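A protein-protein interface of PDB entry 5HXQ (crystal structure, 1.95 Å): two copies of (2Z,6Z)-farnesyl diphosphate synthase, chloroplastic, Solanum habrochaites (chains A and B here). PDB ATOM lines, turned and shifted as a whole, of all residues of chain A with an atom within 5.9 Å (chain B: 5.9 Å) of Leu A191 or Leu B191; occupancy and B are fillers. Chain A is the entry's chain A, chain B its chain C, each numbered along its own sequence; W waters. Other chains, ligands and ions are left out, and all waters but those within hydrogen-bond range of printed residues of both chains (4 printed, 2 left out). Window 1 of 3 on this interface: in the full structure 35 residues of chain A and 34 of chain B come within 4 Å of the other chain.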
ATOM      1  N   TYR A 131      10.072  20.951  11.438  1.00  0.00           N
ATOM      2  CA  TYR A 131       8.668  21.221  11.210  1.00  0.00           C
ATOM      3  C   TYR A 131       8.525  22.227  10.109  1.00  0.00           C
ATOM      4  O   TYR A 131       9.346  23.128   9.974  1.00  0.00           O
ATOM      5  CB  TYR A 131       8.027  21.828  12.469  1.00  0.00           C
ATOM      6  CG  TYR A 131       6.568  22.223  12.275  1.00  0.00           C
ATOM      7  CD1 TYR A 131       5.548  21.301  12.480  1.00  0.00           C
ATOM      8  CD2 TYR A 131       6.221  23.503  11.861  1.00  0.00           C
ATOM      9  CE1 TYR A 131       4.211  21.645  12.294  1.00  0.00           C
ATOM     10  CE2 TYR A 131       4.889  23.860  11.659  1.00  0.00           C
ATOM     11  CZ  TYR A 131       3.882  22.938  11.883  1.00  0.00           C
ATOM     12  OH  TYR A 131       2.547  23.288  11.689  1.00  0.00           O
ATOM     13  N   GLY A 133       4.895  24.262   8.116  1.00  0.00           N
ATOM     14  CA  GLY A 133       3.447  24.377   7.954  1.00  0.00           C
ATOM     15  C   GLY A 133       2.923  23.621   6.758  1.00  0.00           C
ATOM     16  O   GLY A 133       1.885  22.952   6.871  1.00  0.00           O
ATOM     17  N   TYR A 134       3.636  23.681   5.621  1.00  0.00           N
ATOM     18  CA  TYR A 134       3.247  22.883   4.460  1.00  0.00           C
ATOM     19  C   TYR A 134       3.156  21.405   4.832  1.00  0.00           C
ATOM     20  O   TYR A 134       2.207  20.699   4.488  1.00  0.00           O
ATOM     21  CB  TYR A 134       4.293  22.938   3.342  1.00  0.00           C
ATOM     22  CG  TYR A 134       4.569  24.287   2.726  1.00  0.00           C
ATOM     23  CD1 TYR A 134       3.552  25.185   2.431  1.00  0.00           C
ATOM     24  CD2 TYR A 134       5.872  24.644   2.405  1.00  0.00           C
ATOM     25  CE1 TYR A 134       3.839  26.418   1.847  1.00  0.00           C
ATOM     26  CE2 TYR A 134       6.164  25.854   1.818  1.00  0.00           C
ATOM     27  CZ  TYR A 134       5.162  26.738   1.541  1.00  0.00           C
ATOM     28  OH  TYR A 134       5.508  27.947   0.953  1.00  0.00           O
ATOM     29  N   ILE A 137       0.241  20.417   7.013  1.00  0.00           N
ATOM     30  CA  ILE A 137      -0.974  20.385   6.220  1.00  0.00           C
ATOM     31  C   ILE A 137      -0.981  19.175   5.277  1.00  0.00           C
ATOM     32  O   ILE A 137      -2.034  18.548   5.076  1.00  0.00           O
ATOM     33  CB  ILE A 137      -1.159  21.699   5.425  1.00  0.00           C
ATOM     34  CG1 ILE A 137      -1.503  22.843   6.393  1.00  0.00           C
ATOM     35  CG2 ILE A 137      -2.250  21.549   4.376  1.00  0.00           C
ATOM     36  CD1 ILE A 137      -1.344  24.249   5.841  1.00  0.00           C
ATOM     37  N   VAL A 186       6.479  34.584   8.534  1.00  0.00           N
ATOM     38  CA  VAL A 186       6.247  33.400   9.373  1.00  0.00           C
ATOM     39  C   VAL A 186       7.164  32.216   8.991  1.00  0.00           C
ATOM     40  O   VAL A 186       7.284  31.244   9.751  1.00  0.00           O
ATOM     41  CB  VAL A 186       4.760  33.003   9.389  1.00  0.00           C
ATOM     42  CG1 VAL A 186       3.918  34.160   9.878  1.00  0.00           C
ATOM     43  CG2 VAL A 186       4.281  32.568   8.017  1.00  0.00           C
ATOM     44  N   SER A 187       7.825  32.308   7.833  1.00  0.00           N
ATOM     45  CA  SER A 187       8.813  31.318   7.398  1.00  0.00           C
ATOM     46  C   SER A 187       8.324  29.852   7.537  1.00  0.00           C
ATOM     47  O   SER A 187       9.004  29.008   8.095  1.00  0.00           O
ATOM     48  CB  SER A 187      10.159  31.560   8.111  1.00  0.00           C
ATOM     49  OG  SER A 187      10.675  32.861   7.799  1.00  0.00           O
ATOM     50  N   ASN A 188       7.148  29.564   6.991  1.00  0.00           N
ATOM     51  CA  ASN A 188       6.591  28.212   6.986  1.00  0.00           C
ATOM     52  C   ASN A 188       6.501  27.569   8.391  1.00  0.00           C
ATOM     53  O   ASN A 188       6.790  26.400   8.562  1.00  0.00           O
ATOM     54  CB  ASN A 188       7.402  27.313   6.037  1.00  0.00           C
ATOM     55  CG  ASN A 188       6.685  26.024   5.697  1.00  0.00           C
ATOM     56  OD1 ASN A 188       5.459  25.975   5.680  1.00  0.00           O
ATOM     57  ND2 ASN A 188       7.449  24.980   5.402  1.00  0.00           N
ATOM     58  N   PHE A 189       6.077  28.362   9.372  1.00  0.00           N
ATOM     59  CA  PHE A 189       5.783  27.898  10.718  1.00  0.00           C
ATOM     60  C   PHE A 189       4.317  27.448  10.650  1.00  0.00           C
ATOM     61  O   PHE A 189       3.930  26.863   9.647  1.00  0.00           O
ATOM     62  CB  PHE A 189       6.038  29.044  11.720  1.00  0.00           C
ATOM     63  CG  PHE A 189       6.021  28.634  13.190  1.00  0.00           C
ATOM     64  CD1 PHE A 189       6.333  27.339  13.617  1.00  0.00           C
ATOM     65  CD2 PHE A 189       5.724  29.583  14.138  1.00  0.00           C
ATOM     66  CE1 PHE A 189       6.332  27.021  14.968  1.00  0.00           C
ATOM     67  CE2 PHE A 189       5.734  29.281  15.487  1.00  0.00           C
ATOM     68  CZ  PHE A 189       6.029  27.996  15.906  1.00  0.00           C
ATOM     69  N   LEU A 190       3.493  27.785  11.641  1.00  0.00           N
ATOM     70  CA  LEU A 190       2.147  27.216  11.791  1.00  0.00           C
ATOM     71  C   LEU A 190       1.068  27.847  10.907  1.00  0.00           C
ATOM     72  O   LEU A 190       0.189  28.572  11.418  1.00  0.00           O
ATOM     73  CB  LEU A 190       1.703  27.419  13.236  1.00  0.00           C
ATOM     74  CG  LEU A 190       2.646  26.973  14.346  1.00  0.00           C
ATOM     75  CD1 LEU A 190       2.177  27.563  15.672  1.00  0.00           C
ATOM     76  CD2 LEU A 190       2.722  25.457  14.428  1.00  0.00           C
ATOM     77  N   LEU A 191       1.067  27.544   9.616  1.00  0.00           N
ATOM     78  CA  LEU A 191       0.258  28.302   8.650  1.00  0.00           C
ATOM     79  C   LEU A 191      -1.263  28.276   8.915  1.00  0.00           C
ATOM     80  O   LEU A 191      -1.908  29.326   8.993  1.00  0.00           O
ATOM     81  CB  LEU A 191       0.557  27.827   7.232  1.00  0.00           C
ATOM     82  CG  LEU A 191       2.020  27.924   6.783  1.00  0.00           C
ATOM     83  CD1 LEU A 191       2.210  27.358   5.391  1.00  0.00           C
ATOM     84  CD2 LEU A 191       2.507  29.363   6.861  1.00  0.00           C
ATOM     85  N   TRP A 192      -1.817  27.078   9.064  1.00  0.00           N
ATOM     86  CA  TRP A 192      -3.244  26.914   9.328  1.00  0.00           C
ATOM     87  C   TRP A 192      -3.608  27.548  10.664  1.00  0.00           C
ATOM     88  O   TRP A 192      -4.577  28.290  10.747  1.00  0.00           O
ATOM     89  CB  TRP A 192      -3.596  25.420   9.330  1.00  0.00           C
ATOM     90  CG  TRP A 192      -4.991  25.091   9.699  1.00  0.00           C
ATOM     91  CD1 TRP A 192      -5.501  24.978  10.973  1.00  0.00           C
ATOM     92  CD2 TRP A 192      -6.066  24.772   8.808  1.00  0.00           C
ATOM     93  NE1 TRP A 192      -6.820  24.632  10.916  1.00  0.00           N
ATOM     94  CE2 TRP A 192      -7.195  24.484   9.608  1.00  0.00           C
ATOM     95  CE3 TRP A 192      -6.192  24.717   7.416  1.00  0.00           C
ATOM     96  CZ2 TRP A 192      -8.435  24.153   9.062  1.00  0.00           C
ATOM     97  CZ3 TRP A 192      -7.432  24.361   6.873  1.00  0.00           C
ATOM     98  CH2 TRP A 192      -8.534  24.093   7.700  1.00  0.00           C
ATOM     99  N   GLN A 193      -2.754  27.316  11.654  1.00  0.00           N
ATOM    100  CA  GLN A 193      -3.008  27.668  13.033  1.00  0.00           C
ATOM    101  C   GLN A 193      -2.890  29.172  13.312  1.00  0.00           C
ATOM    102  O   GLN A 193      -3.374  29.639  14.329  1.00  0.00           O
ATOM    103  CB  GLN A 193      -2.068  26.895  13.957  1.00  0.00           C
ATOM    104  CG  GLN A 193      -2.209  25.373  13.944  1.00  0.00           C
ATOM    105  CD  GLN A 193      -1.381  24.666  12.862  1.00  0.00           C
ATOM    106  OE1 GLN A 193      -0.854  25.285  11.933  1.00  0.00           O
ATOM    107  NE2 GLN A 193      -1.280  23.347  12.981  1.00  0.00           N
ATOM    108  N   LEU A 194      -2.260  29.923  12.419  1.00  0.00           N
ATOM    109  CA  LEU A 194      -2.057  31.356  12.613  1.00  0.00           C
ATOM    110  C   LEU A 194      -3.101  32.245  11.937  1.00  0.00           C
ATOM    111  O   LEU A 194      -2.866  33.447  11.745  1.00  0.00           O
ATOM    112  CB  LEU A 194      -0.646  31.754  12.134  1.00  0.00           C
ATOM    113  CG  LEU A 194       0.514  31.164  12.943  1.00  0.00           C
ATOM    114  CD1 LEU A 194       1.846  31.412  12.251  1.00  0.00           C
ATOM    115  CD2 LEU A 194       0.565  31.709  14.358  1.00  0.00           C
ATOM    116  N   ALA A 195      -4.248  31.680  11.582  1.00  0.00           N
ATOM    117  CA  ALA A 195      -5.258  32.404  10.804  1.00  0.00           C
ATOM    118  C   ALA A 195      -5.776  33.698  11.465  1.00  0.00           C
ATOM    119  O   ALA A 195      -6.026  34.677  10.771  1.00  0.00           O
ATOM    120  CB  ALA A 195      -6.416  31.475  10.477  1.00  0.00           C
ATOM    121  N   TYR B 131     -13.931  34.401   0.219  1.00  0.00           N
ATOM    122  CA  TYR B 131     -12.768  33.528   0.221  1.00  0.00           C
ATOM    123  C   TYR B 131     -12.221  33.440   1.627  1.00  0.00           C
ATOM    124  O   TYR B 131     -12.388  34.359   2.437  1.00  0.00           O
ATOM    125  CB  TYR B 131     -11.704  34.081  -0.738  1.00  0.00           C
ATOM    126  CG  TYR B 131     -10.354  33.384  -0.648  1.00  0.00           C
ATOM    127  CD1 TYR B 131      -9.997  32.394  -1.555  1.00  0.00           C
ATOM    128  CD2 TYR B 131      -9.432  33.734   0.348  1.00  0.00           C
ATOM    129  CE1 TYR B 131      -8.762  31.756  -1.470  1.00  0.00           C
ATOM    130  CE2 TYR B 131      -8.210  33.099   0.448  1.00  0.00           C
ATOM    131  CZ  TYR B 131      -7.878  32.115  -0.467  1.00  0.00           C
ATOM    132  OH  TYR B 131      -6.660  31.497  -0.374  1.00  0.00           O
ATOM    133  N   GLY B 132     -11.546  32.333   1.908  1.00  0.00           N
ATOM    134  CA  GLY B 132     -10.790  32.190   3.143  1.00  0.00           C
ATOM    135  C   GLY B 132      -9.675  31.179   2.966  1.00  0.00           C
ATOM    136  O   GLY B 132      -9.728  30.349   2.080  1.00  0.00           O
ATOM    137  N   GLY B 133      -8.653  31.279   3.799  1.00  0.00           N
ATOM    138  CA  GLY B 133      -7.544  30.343   3.776  1.00  0.00           C
ATOM    139  C   GLY B 133      -7.975  28.929   4.112  1.00  0.00           C
ATOM    140  O   GLY B 133      -7.589  27.985   3.424  1.00  0.00           O
ATOM    141  N   TYR B 134      -8.783  28.791   5.162  1.00  0.00           N
ATOM    142  CA  TYR B 134      -9.376  27.496   5.499  1.00  0.00           C
ATOM    143  C   TYR B 134     -10.129  26.947   4.296  1.00  0.00           C
ATOM    144  O   TYR B 134      -9.928  25.801   3.890  1.00  0.00           O
ATOM    145  CB  TYR B 134     -10.373  27.611   6.646  1.00  0.00           C
ATOM    146  CG  TYR B 134      -9.864  28.097   7.976  1.00  0.00           C
ATOM    147  CD1 TYR B 134      -8.626  27.697   8.495  1.00  0.00           C
ATOM    148  CD2 TYR B 134     -10.662  28.915   8.757  1.00  0.00           C
ATOM    149  CE1 TYR B 134      -8.210  28.122   9.741  1.00  0.00           C
ATOM    150  CE2 TYR B 134     -10.245  29.357   9.990  1.00  0.00           C
ATOM    151  CZ  TYR B 134      -9.027  28.963  10.477  1.00  0.00           C
ATOM    152  OH  TYR B 134      -8.670  29.424  11.718  1.00  0.00           O
ATOM    153  N   ILE B 137      -7.790  25.650   1.348  1.00  0.00           N
ATOM    154  CA  ILE B 137      -7.152  24.396   1.725  1.00  0.00           C
ATOM    155  C   ILE B 137      -8.169  23.240   1.726  1.00  0.00           C
ATOM    156  O   ILE B 137      -7.866  22.151   1.248  1.00  0.00           O
ATOM    157  CB  ILE B 137      -6.437  24.529   3.088  1.00  0.00           C
ATOM    158  CG1 ILE B 137      -5.165  25.385   2.923  1.00  0.00           C
ATOM    159  CG2 ILE B 137      -6.052  23.178   3.657  1.00  0.00           C
ATOM    160  CD1 ILE B 137      -4.612  25.937   4.217  1.00  0.00           C
ATOM    161  N   VAL B 186      -3.701  38.190   9.797  1.00  0.00           N
ATOM    162  CA  VAL B 186      -3.994  37.882   8.398  1.00  0.00           C
ATOM    163  C   VAL B 186      -5.468  37.526   8.202  1.00  0.00           C
ATOM    164  O   VAL B 186      -5.925  37.436   7.074  1.00  0.00           O
ATOM    165  CB  VAL B 186      -3.070  36.774   7.824  1.00  0.00           C
ATOM    166  CG1 VAL B 186      -1.617  37.195   7.938  1.00  0.00           C
ATOM    167  CG2 VAL B 186      -3.278  35.425   8.510  1.00  0.00           C
ATOM    168  N   ASN B 188      -7.465  34.945   8.232  1.00  0.00           N
ATOM    169  CA  ASN B 188      -7.871  33.875   7.335  1.00  0.00           C
ATOM    170  C   ASN B 188      -7.887  34.282   5.850  1.00  0.00           C
ATOM    171  O   ASN B 188      -8.755  33.876   5.078  1.00  0.00           O
ATOM    172  CB  ASN B 188      -9.238  33.344   7.768  1.00  0.00           C
ATOM    173  CG  ASN B 188      -9.616  32.054   7.080  1.00  0.00           C
ATOM    174  OD1 ASN B 188      -8.758  31.227   6.777  1.00  0.00           O
ATOM    175  ND2 ASN B 188     -10.921  31.866   6.842  1.00  0.00           N
ATOM    176  N   PHE B 189      -6.895  35.070   5.459  1.00  0.00           N
ATOM    177  CA  PHE B 189      -6.629  35.372   4.062  1.00  0.00           C
ATOM    178  C   PHE B 189      -5.775  34.192   3.503  1.00  0.00           C
ATOM    179  O   PHE B 189      -6.091  33.057   3.765  1.00  0.00           O
ATOM    180  CB  PHE B 189      -5.943  36.745   3.999  1.00  0.00           C
ATOM    181  CG  PHE B 189      -5.865  37.361   2.637  1.00  0.00           C
ATOM    182  CD1 PHE B 189      -6.794  37.082   1.644  1.00  0.00           C
ATOM    183  CD2 PHE B 189      -4.877  38.286   2.364  1.00  0.00           C
ATOM    184  CE1 PHE B 189      -6.692  37.674   0.404  1.00  0.00           C
ATOM    185  CE2 PHE B 189      -4.779  38.890   1.128  1.00  0.00           C
ATOM    186  CZ  PHE B 189      -5.694  38.590   0.149  1.00  0.00           C
ATOM    187  N   LEU B 190      -4.691  34.439   2.777  1.00  0.00           N
ATOM    188  CA  LEU B 190      -4.028  33.405   1.965  1.00  0.00           C
ATOM    189  C   LEU B 190      -3.023  32.556   2.742  1.00  0.00           C
ATOM    190  O   LEU B 190      -1.794  32.642   2.475  1.00  0.00           O
ATOM    191  CB  LEU B 190      -3.281  34.083   0.817  1.00  0.00           C
ATOM    192  CG  LEU B 190      -4.020  35.074  -0.062  1.00  0.00           C
ATOM    193  CD1 LEU B 190      -3.053  35.751  -1.033  1.00  0.00           C
ATOM    194  CD2 LEU B 190      -5.150  34.367  -0.799  1.00  0.00           C
ATOM    195  N   LEU B 191      -3.518  31.713   3.663  1.00  0.00           N
ATOM    196  CA  LEU B 191      -2.671  31.034   4.666  1.00  0.00           C
ATOM    197  C   LEU B 191      -1.478  30.230   4.087  1.00  0.00           C
ATOM    198  O   LEU B 191      -0.325  30.505   4.403  1.00  0.00           O
ATOM    199  CB  LEU B 191      -3.537  30.132   5.564  1.00  0.00           C
ATOM    200  CG  LEU B 191      -4.666  30.825   6.355  1.00  0.00           C
ATOM    201  CD1 LEU B 191      -5.607  29.789   6.951  1.00  0.00           C
ATOM    202  CD2 LEU B 191      -4.110  31.735   7.435  1.00  0.00           C
ATOM    203  N   TRP B 192      -1.762  29.250   3.241  1.00  0.00           N
ATOM    204  CA  TRP B 192      -0.708  28.449   2.613  1.00  0.00           C
ATOM    205  C   TRP B 192       0.270  29.334   1.841  1.00  0.00           C
ATOM    206  O   TRP B 192       1.479  29.192   1.975  1.00  0.00           O
ATOM    207  CB  TRP B 192      -1.341  27.419   1.694  1.00  0.00           C
ATOM    208  CG  TRP B 192      -0.393  26.598   0.843  1.00  0.00           C
ATOM    209  CD1 TRP B 192       0.166  26.955  -0.356  1.00  0.00           C
ATOM    210  CD2 TRP B 192       0.013  25.258   1.092  1.00  0.00           C
ATOM    211  NE1 TRP B 192       0.927  25.919  -0.850  1.00  0.00           N
ATOM    212  CE2 TRP B 192       0.844  24.863   0.017  1.00  0.00           C
ATOM    213  CE3 TRP B 192      -0.232  24.349   2.124  1.00  0.00           C
ATOM    214  CZ2 TRP B 192       1.430  23.605  -0.045  1.00  0.00           C
ATOM    215  CZ3 TRP B 192       0.347  23.104   2.059  1.00  0.00           C
ATOM    216  CH2 TRP B 192       1.168  22.739   0.976  1.00  0.00           C
ATOM    217  N   GLN B 193      -0.295  30.285   1.110  1.00  0.00           N
ATOM    218  CA  GLN B 193       0.411  31.126   0.175  1.00  0.00           C
ATOM    219  C   GLN B 193       1.283  32.205   0.854  1.00  0.00           C
ATOM    220  O   GLN B 193       2.172  32.763   0.215  1.00  0.00           O
ATOM    221  CB  GLN B 193      -0.592  31.773  -0.794  1.00  0.00           C
ATOM    222  CG  GLN B 193      -1.369  30.792  -1.658  1.00  0.00           C
ATOM    223  CD  GLN B 193      -2.686  30.327  -1.029  1.00  0.00           C
ATOM    224  OE1 GLN B 193      -2.921  30.466   0.191  1.00  0.00           O
ATOM    225  NE2 GLN B 193      -3.543  29.757  -1.851  1.00  0.00           N
ATOM    226  N   LEU B 194       1.063  32.454   2.143  1.00  0.00           N
ATOM    227  CA  LEU B 194       1.805  33.467   2.891  1.00  0.00           C
ATOM    228  C   LEU B 194       2.993  32.930   3.657  1.00  0.00           C
ATOM    229  O   LEU B 194       3.530  33.644   4.470  1.00  0.00           O
ATOM    230  CB  LEU B 194       0.868  34.209   3.890  1.00  0.00           C
ATOM    231  CG  LEU B 194      -0.267  35.041   3.274  1.00  0.00           C
ATOM    232  CD1 LEU B 194      -1.180  35.679   4.330  1.00  0.00           C
ATOM    233  CD2 LEU B 194       0.279  36.117   2.352  1.00  0.00           C
ATOM    234  N   ALA B 195       3.403  31.680   3.406  1.00  0.00           N
ATOM    235  CA  ALA B 195       4.451  31.031   4.190  1.00  0.00           C
ATOM    236  C   ALA B 195       5.757  31.819   4.244  1.00  0.00           C
ATOM    237  O   ALA B 195       6.432  31.792   5.251  1.00  0.00           O
ATOM    238  CB  ALA B 195       4.726  29.622   3.665  1.00  0.00           C
HETATM  239  O   HOH W   1       3.560  29.434   0.325  1.00  0.00           O
HETATM  240  O   HOH W   2      -0.250  31.707   7.529  1.00  0.00           O
HETATM  241  O   HOH W   3      -6.525  28.503  12.637  1.00  0.00           O
HETATM  242  O   HOH W   4       5.677  34.875   5.873  1.00  0.00           O
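The backbone NH of Asn A188 sits at hydrogen-bond distance from the backbone carbonyl oxygen of Ala B195 (2.9 Å). N of Ser A187 lies within hydrogen-bond range of O of Ala B195 (3.0 Å). The backbone carbonyl oxygen of Ala A195 lies within hydrogen-bond range of the backbone NH of Asn B188, 2.9 Å away.
OD1 of Asn B188 sits at hydrogen-bond distance from N of Tyr B134 (2.9 Å). The backbone carbonyl oxygen (O) of Asn B188 is in hydrogen-bond range of the backbone NH (N) of Gly B133, 2.9 Å away. The backbone NH (N) of Gly A133 is in hydrogen-bond range of the backbone carbonyl oxygen (O) of Asn A188 (2.9 Å). The backbone NH of Tyr A134 is in hydrogen-bond range of the side-chain amide oxygen of Asn A188.
Trp B192 touches Tyr A134. Ile A137 touches Trp B192 (CG2 to CZ3, 3.8 Å). Val A186 touches Leu B194. Val A186 touches Ala B195. O of Trp B192 touches CD1 of Leu A191, at 3.9 Å. Trp A192 touches Tyr B134 (CZ2 to CD1, 3.6 Å). CG2 of Val B186 touches O of Leu A194, at 3.8 Å. Tyr B134 touches Ala A195 (OH to CB, 3.3 Å). O of Ala A195 touches CG2 of Val B186, at 3.6 Å. Ala A195 touches Leu B191 (CA to CD2, 3.6 Å).
Leu A191 touches just these residues of chain B: Leu B191 (3.6 Å), Trp B192 (3.9 Å) and Ala B195 (3.7 Å). Of chain A, only Leu A191 (3.6 Å) and Ala A195 (3.6 Å) come within 4 Å of Leu B191. Of the printed residues of chain B, Ile A137 touches Trp B192. Printed residues of chain A within 4 Å of Tyr B134: Trp A192 and Ala A195. Printed residues of chain B within 4 Å of Trp A192: Tyr B134 (3.6 Å) and Ile B137 (3.7 Å). Gln A193 touches none of the printed residues of chain B. Leu A190 touches none of the printed residues of chain B. The nearest residue of chain B that does not touch Leu A191 is Leu B194 (4.8 Å). The nearest residue of chain A that does not touch Leu B191 is Trp A192 (4.2 Å). The nearest printed residue of chain B that does not touch Ser A187 is Leu B194 (5.6 Å).
Printed residues of chain B that touch a printed residue of chain A: Tyr B134, Ile B137, Val B186, Asn B188, Leu B191, Trp B192, Leu B194 and Ala B195. Of the 14 printed residues of chain A, 9 touch a printed residue of chain B. Among the printed residues, no Asp or Glu carboxylate lies within 4 Å of a Lys or Arg side-chain nitrogen of the other chain.
Val A186 touches Leu B194, and with the chains exchanged Leu A194 touches Val B186. Val A186 touches Ala B195, and with the chains exchanged Ala A195 touches Val B186. Asn A188 touches Ala B195, and with the chains exchanged Ala A195 touches Asn B188. Leu B191 touches its own counterpart, Leu A191.
Water W3 lies within hydrogen-bond range of the side-chain hydroxyl (OH) of Tyr B134 (2.5 Å) and the backbone carbonyl oxygen (O) of Trp A192 (2.7 Å). Water W1 bridges OH of Tyr A134 (2.5 Å) and O of Trp B192 (2.7 Å). Water W4 lies within hydrogen-bond range of the backbone NH (N) of Val A186 (2.8 Å), the backbone carbonyl oxygen (O) of Leu B194 (2.8 Å) and the backbone carbonyl oxygen (O) of Ala B195 (3.2 Å). Water W2 lies within hydrogen-bond range of the backbone carbonyl oxygen of Leu A191 (3.2 Å) and the backbone carbonyl oxygen of Leu B191 (3.3 Å).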
